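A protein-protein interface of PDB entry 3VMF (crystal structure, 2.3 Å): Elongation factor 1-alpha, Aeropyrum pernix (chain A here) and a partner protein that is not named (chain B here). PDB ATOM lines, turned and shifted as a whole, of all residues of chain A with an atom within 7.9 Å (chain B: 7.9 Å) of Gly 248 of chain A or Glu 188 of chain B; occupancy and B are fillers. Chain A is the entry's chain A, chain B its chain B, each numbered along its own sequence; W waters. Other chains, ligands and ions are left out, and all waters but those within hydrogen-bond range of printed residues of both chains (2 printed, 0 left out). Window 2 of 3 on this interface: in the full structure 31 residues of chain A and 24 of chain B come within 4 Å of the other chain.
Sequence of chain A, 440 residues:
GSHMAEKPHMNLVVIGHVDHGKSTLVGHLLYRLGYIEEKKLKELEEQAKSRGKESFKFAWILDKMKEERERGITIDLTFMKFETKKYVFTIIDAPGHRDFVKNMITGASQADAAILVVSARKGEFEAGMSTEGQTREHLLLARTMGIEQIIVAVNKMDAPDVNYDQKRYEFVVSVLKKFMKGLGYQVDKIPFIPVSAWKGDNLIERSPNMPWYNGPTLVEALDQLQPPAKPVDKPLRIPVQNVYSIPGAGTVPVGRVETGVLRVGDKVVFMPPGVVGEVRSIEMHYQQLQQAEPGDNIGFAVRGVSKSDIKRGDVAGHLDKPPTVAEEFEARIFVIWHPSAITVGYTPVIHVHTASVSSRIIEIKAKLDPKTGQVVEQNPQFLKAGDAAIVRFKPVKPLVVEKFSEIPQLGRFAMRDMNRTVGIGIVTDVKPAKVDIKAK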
ATOM      1  N   SER A 245     -22.200 -20.146  18.931  1.00  0.00           N
ATOM      2  CA  SER A 245     -22.164 -20.507  17.518  1.00  0.00           C
ATOM      3  C   SER A 245     -20.829 -21.160  17.294  1.00  0.00           C
ATOM      4  O   SER A 245     -19.796 -20.505  17.375  1.00  0.00           O
ATOM      5  CB  SER A 245     -22.276 -19.270  16.633  1.00  0.00           C
ATOM      6  OG  SER A 245     -22.257 -19.639  15.272  1.00  0.00           O
ATOM      7  N   ILE A 246     -20.836 -22.460  17.048  1.00  0.00           N
ATOM      8  CA  ILE A 246     -19.617 -23.230  17.235  1.00  0.00           C
ATOM      9  C   ILE A 246     -19.216 -23.980  15.980  1.00  0.00           C
ATOM     10  O   ILE A 246     -20.028 -24.713  15.409  1.00  0.00           O
ATOM     11  CB  ILE A 246     -19.752 -24.197  18.423  1.00  0.00           C
ATOM     12  CG1 ILE A 246     -20.071 -23.422  19.698  1.00  0.00           C
ATOM     13  CG2 ILE A 246     -18.482 -25.019  18.607  1.00  0.00           C
ATOM     14  CD1 ILE A 246     -19.839 -24.219  20.964  1.00  0.00           C
ATOM     15  N   PRO A 247     -17.959 -23.775  15.540  1.00  0.00           N
ATOM     16  CA  PRO A 247     -17.427 -24.410  14.335  1.00  0.00           C
ATOM     17  C   PRO A 247     -17.538 -25.912  14.463  1.00  0.00           C
ATOM     18  O   PRO A 247     -16.950 -26.487  15.380  1.00  0.00           O
ATOM     19  CB  PRO A 247     -15.953 -23.978  14.334  1.00  0.00           C
ATOM     20  CG  PRO A 247     -15.917 -22.721  15.103  1.00  0.00           C
ATOM     21  CD  PRO A 247     -16.961 -22.890  16.175  1.00  0.00           C
ATOM     22  N   GLY A 248     -18.296 -26.532  13.565  1.00  0.00           N
ATOM     23  CA  GLY A 248     -18.559 -27.954  13.656  1.00  0.00           C
ATOM     24  C   GLY A 248     -19.982 -28.263  14.098  1.00  0.00           C
ATOM     25  O   GLY A 248     -20.643 -29.143  13.535  1.00  0.00           O
ATOM     26  N   ALA A 249     -20.471 -27.532  15.098  1.00  0.00           N
ATOM     27  CA  ALA A 249     -21.790 -27.816  15.651  1.00  0.00           C
ATOM     28  C   ALA A 249     -22.847 -26.915  15.049  1.00  0.00           C
ATOM     29  O   ALA A 249     -23.954 -27.353  14.731  1.00  0.00           O
ATOM     30  CB  ALA A 249     -21.774 -27.675  17.174  1.00  0.00           C
ATOM     31  N   GLY A 250     -22.497 -25.647  14.890  1.00  0.00           N
ATOM     32  CA  GLY A 250     -23.463 -24.665  14.458  1.00  0.00           C
ATOM     33  C   GLY A 250     -23.922 -23.873  15.664  1.00  0.00           C
ATOM     34  O   GLY A 250     -23.123 -23.504  16.525  1.00  0.00           O
ATOM     35  N   THR A 251     -25.212 -23.596  15.743  1.00  0.00           N
ATOM     36  CA  THR A 251     -25.688 -22.829  16.892  1.00  0.00           C
ATOM     37  C   THR A 251     -26.133 -23.725  18.052  1.00  0.00           C
ATOM     38  O   THR A 251     -27.012 -24.581  17.923  1.00  0.00           O
ATOM     39  CB  THR A 251     -26.726 -21.801  16.473  1.00  0.00           C
ATOM     40  OG1 THR A 251     -27.836 -21.790  17.382  1.00  0.00           O
ATOM     41  CG2 THR A 251     -27.176 -22.147  15.145  1.00  0.00           C
ATOM     42  N   VAL A 252     -25.463 -23.550  19.179  1.00  0.00           N
ATOM     43  CA  VAL A 252     -25.737 -24.381  20.323  1.00  0.00           C
ATOM     44  C   VAL A 252     -26.227 -23.556  21.513  1.00  0.00           C
ATOM     45  O   VAL A 252     -25.474 -22.811  22.151  1.00  0.00           O
ATOM     46  CB  VAL A 252     -24.564 -25.375  20.622  1.00  0.00           C
ATOM     47  CG1 VAL A 252     -23.339 -25.014  19.827  1.00  0.00           C
ATOM     48  CG2 VAL A 252     -24.261 -25.506  22.117  1.00  0.00           C
ATOM     49  N   ARG A 280     -28.548 -32.187  16.751  1.00  0.00           N
ATOM     50  CA  ARG A 280     -27.462 -32.913  16.095  1.00  0.00           C
ATOM     51  C   ARG A 280     -26.653 -33.638  17.155  1.00  0.00           C
ATOM     52  O   ARG A 280     -26.091 -34.715  16.921  1.00  0.00           O
ATOM     53  CB  ARG A 280     -26.481 -31.945  15.426  1.00  0.00           C
ATOM     54  CG  ARG A 280     -26.954 -31.186  14.215  1.00  0.00           C
ATOM     55  CD  ARG A 280     -25.862 -30.184  13.820  1.00  0.00           C
ATOM     56  NE  ARG A 280     -26.234 -29.337  12.689  1.00  0.00           N
ATOM     57  CZ  ARG A 280     -25.688 -29.425  11.477  1.00  0.00           C
ATOM     58  NH1 ARG A 280     -24.731 -30.321  11.240  1.00  0.00           N
ATOM     59  NH2 ARG A 280     -26.091 -28.608  10.505  1.00  0.00           N
ATOM     60  N   SER A 281     -26.554 -33.002  18.315  1.00  0.00           N
ATOM     61  CA  SER A 281     -25.647 -33.463  19.341  1.00  0.00           C
ATOM     62  C   SER A 281     -25.940 -32.796  20.670  1.00  0.00           C
ATOM     63  O   SER A 281     -26.610 -31.751  20.739  1.00  0.00           O
ATOM     64  CB  SER A 281     -24.200 -33.170  18.947  1.00  0.00           C
ATOM     65  OG  SER A 281     -23.899 -31.799  19.128  1.00  0.00           O
ATOM     66  N   ALA A 301     -26.558 -28.778  20.076  1.00  0.00           N
ATOM     67  CA  ALA A 301     -26.492 -28.233  18.711  1.00  0.00           C
ATOM     68  C   ALA A 301     -27.850 -28.330  18.018  1.00  0.00           C
ATOM     69  O   ALA A 301     -28.552 -29.318  18.175  1.00  0.00           O
ATOM     70  CB  ALA A 301     -25.419 -28.946  17.889  1.00  0.00           C
ATOM     71  N   ARG A 303     -29.778 -28.002  14.320  1.00  0.00           N
ATOM     72  CA  ARG A 303     -29.846 -27.852  12.868  1.00  0.00           C
ATOM     73  C   ARG A 303     -31.056 -27.000  12.492  1.00  0.00           C
ATOM     74  O   ARG A 303     -32.130 -27.164  13.051  1.00  0.00           O
ATOM     75  CB  ARG A 303     -29.915 -29.228  12.180  1.00  0.00           C
ATOM     76  CG  ARG A 303     -29.206 -29.296  10.807  1.00  0.00           C
ATOM     77  CD  ARG A 303     -29.060 -30.736  10.264  1.00  0.00           C
ATOM     78  NE  ARG A 303     -27.883 -30.896   9.403  1.00  0.00           N
ATOM     79  CZ  ARG A 303     -26.905 -31.786   9.600  1.00  0.00           C
ATOM     80  NH1 ARG A 303     -26.953 -32.626  10.632  1.00  0.00           N
ATOM     81  NH2 ARG A 303     -25.875 -31.838   8.764  1.00  0.00           N
ATOM     82  N   GLY A 304     -30.872 -26.074  11.558  1.00  0.00           N
ATOM     83  CA  GLY A 304     -31.978 -25.273  11.053  1.00  0.00           C
ATOM     84  C   GLY A 304     -32.347 -24.038  11.864  1.00  0.00           C
ATOM     85  O   GLY A 304     -33.371 -23.405  11.605  1.00  0.00           O
ATOM     86  N   GLU B 188     -23.461 -26.341   7.889  1.00  0.00           N
ATOM     87  CA  GLU B 188     -23.726 -25.638   9.133  1.00  0.00           C
ATOM     88  C   GLU B 188     -23.577 -24.133   9.006  1.00  0.00           C
ATOM     89  O   GLU B 188     -23.025 -23.629   8.032  1.00  0.00           O
ATOM     90  CB  GLU B 188     -22.766 -26.111  10.199  1.00  0.00           C
ATOM     91  CG  GLU B 188     -21.336 -25.802   9.877  1.00  0.00           C
ATOM     92  CD  GLU B 188     -20.416 -26.415  10.889  1.00  0.00           C
ATOM     93  OE1 GLU B 188     -20.849 -27.403  11.519  1.00  0.00           O
ATOM     94  OE2 GLU B 188     -19.282 -25.922  11.072  1.00  0.00           O
ATOM     95  N   ARG B 189     -24.066 -23.424  10.017  1.00  0.00           N
ATOM     96  CA  ARG B 189     -23.988 -21.969  10.065  1.00  0.00           C
ATOM     97  C   ARG B 189     -23.189 -21.511  11.295  1.00  0.00           C
ATOM     98  O   ARG B 189     -23.340 -22.052  12.399  1.00  0.00           O
ATOM     99  CB  ARG B 189     -25.393 -21.349  10.027  1.00  0.00           C
ATOM    100  CG  ARG B 189     -26.348 -21.845  11.145  1.00  0.00           C
ATOM    101  CD  ARG B 189     -27.824 -21.475  10.878  1.00  0.00           C
ATOM    102  NE  ARG B 189     -28.432 -22.353   9.879  1.00  0.00           N
ATOM    103  CZ  ARG B 189     -29.709 -22.306   9.508  1.00  0.00           C
ATOM    104  NH1 ARG B 189     -30.537 -21.427  10.055  1.00  0.00           N
ATOM    105  NH2 ARG B 189     -30.163 -23.151   8.592  1.00  0.00           N
ATOM    106  N   ILE B 190     -22.305 -20.544  11.075  1.00  0.00           N
ATOM    107  CA  ILE B 190     -21.448 -20.004  12.114  1.00  0.00           C
ATOM    108  C   ILE B 190     -21.488 -18.499  12.008  1.00  0.00           C
ATOM    109  O   ILE B 190     -21.322 -17.947  10.916  1.00  0.00           O
ATOM    110  CB  ILE B 190     -19.982 -20.414  11.925  1.00  0.00           C
ATOM    111  CG1 ILE B 190     -19.839 -21.926  11.986  1.00  0.00           C
ATOM    112  CG2 ILE B 190     -19.085 -19.740  12.976  1.00  0.00           C
ATOM    113  CD1 ILE B 190     -18.461 -22.372  11.612  1.00  0.00           C
ATOM    114  N   ILE B 191     -21.704 -17.838  13.139  1.00  0.00           N
ATOM    115  CA  ILE B 191     -21.736 -16.385  13.176  1.00  0.00           C
ATOM    116  C   ILE B 191     -20.980 -15.906  14.408  1.00  0.00           C
ATOM    117  O   ILE B 191     -21.014 -16.533  15.451  1.00  0.00           O
ATOM    118  CB  ILE B 191     -23.182 -15.856  13.127  1.00  0.00           C
ATOM    119  CG1 ILE B 191     -23.201 -14.325  13.003  1.00  0.00           C
ATOM    120  CG2 ILE B 191     -23.970 -16.373  14.321  1.00  0.00           C
ATOM    121  CD1 ILE B 191     -24.511 -13.752  12.433  1.00  0.00           C
HETATM  122  O   HOH W   1     -24.816 -20.409  14.192  1.00  0.00           O
HETATM  123  O   HOH W   2     -21.841 -30.549  11.517  1.00  0.00           O
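The side-chain hydroxyl of Ser 245 of chain A is in hydrogen-bond range of the backbone NH of Ile 191 of chain B (2.8 Å). N of Gly 248 of chain A lies within hydrogen-bond range of OE2 of Glu 188 of chain B.
Among the printed residues, merely in contact across the chains: Ser 245 of chain A with Arg 189 of chain B, Ser 245 of chain A with Ile 190 of chain B, Pro 247 of chain A with Glu 188 of chain B, Pro 247 of chain A with Ile 190 of chain B, Ala 249 of chain A with Glu 188 of chain B, Gly 250 of chain A with Arg 189 of chain B and Gly 304 of chain A with Arg 189 of chain B.
Printed residues of chain B within 4 Å of Ser 245 of chain A: Arg 189, Ile 190 and Ile 191. Gly 248 of chain A touches just one residue of chain B: Glu 188. Of the printed residues of chain B, Gly 250 of chain A touches Arg 189 (3.3 Å). Thr 251 of chain A touches none of the printed residues of chain B. Arg 280 of chain A touches none of the printed residues of chain B. Printed residues of chain B within 4 Å of Gly 304 of chain A: Arg 189 (3.7 Å). Printed residues of chain A within 4 Å of Glu 188 of chain B: Pro 247, Gly 248 and Ala 249. Of the printed residues of chain A, Arg 189 of chain B touches Ser 245, Gly 250 and Gly 304.
Of the 4 printed residues of chain B, 4 touch a printed residue of chain A. Hydrophobic or aromatic side chains of chain B within 4 Å of the printed part of chain A: Ile 190 and Ile 191. Among the printed residues, no Asp or Glu carboxylate lies within 4 Å of a Lys or Arg side-chain nitrogen of the other chain.
Water W2 lies within hydrogen-bond range of O of Gly 248 of chain A (2.7 Å), NH1 of Arg 280 of chain A (2.9 Å) and OE1 of Glu 188 of chain B (3.3 Å). Water W1 bridges the backbone carbonyl oxygen of Arg 189 of chain B and the side-chain hydroxyl of Ser 245 of chain A.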
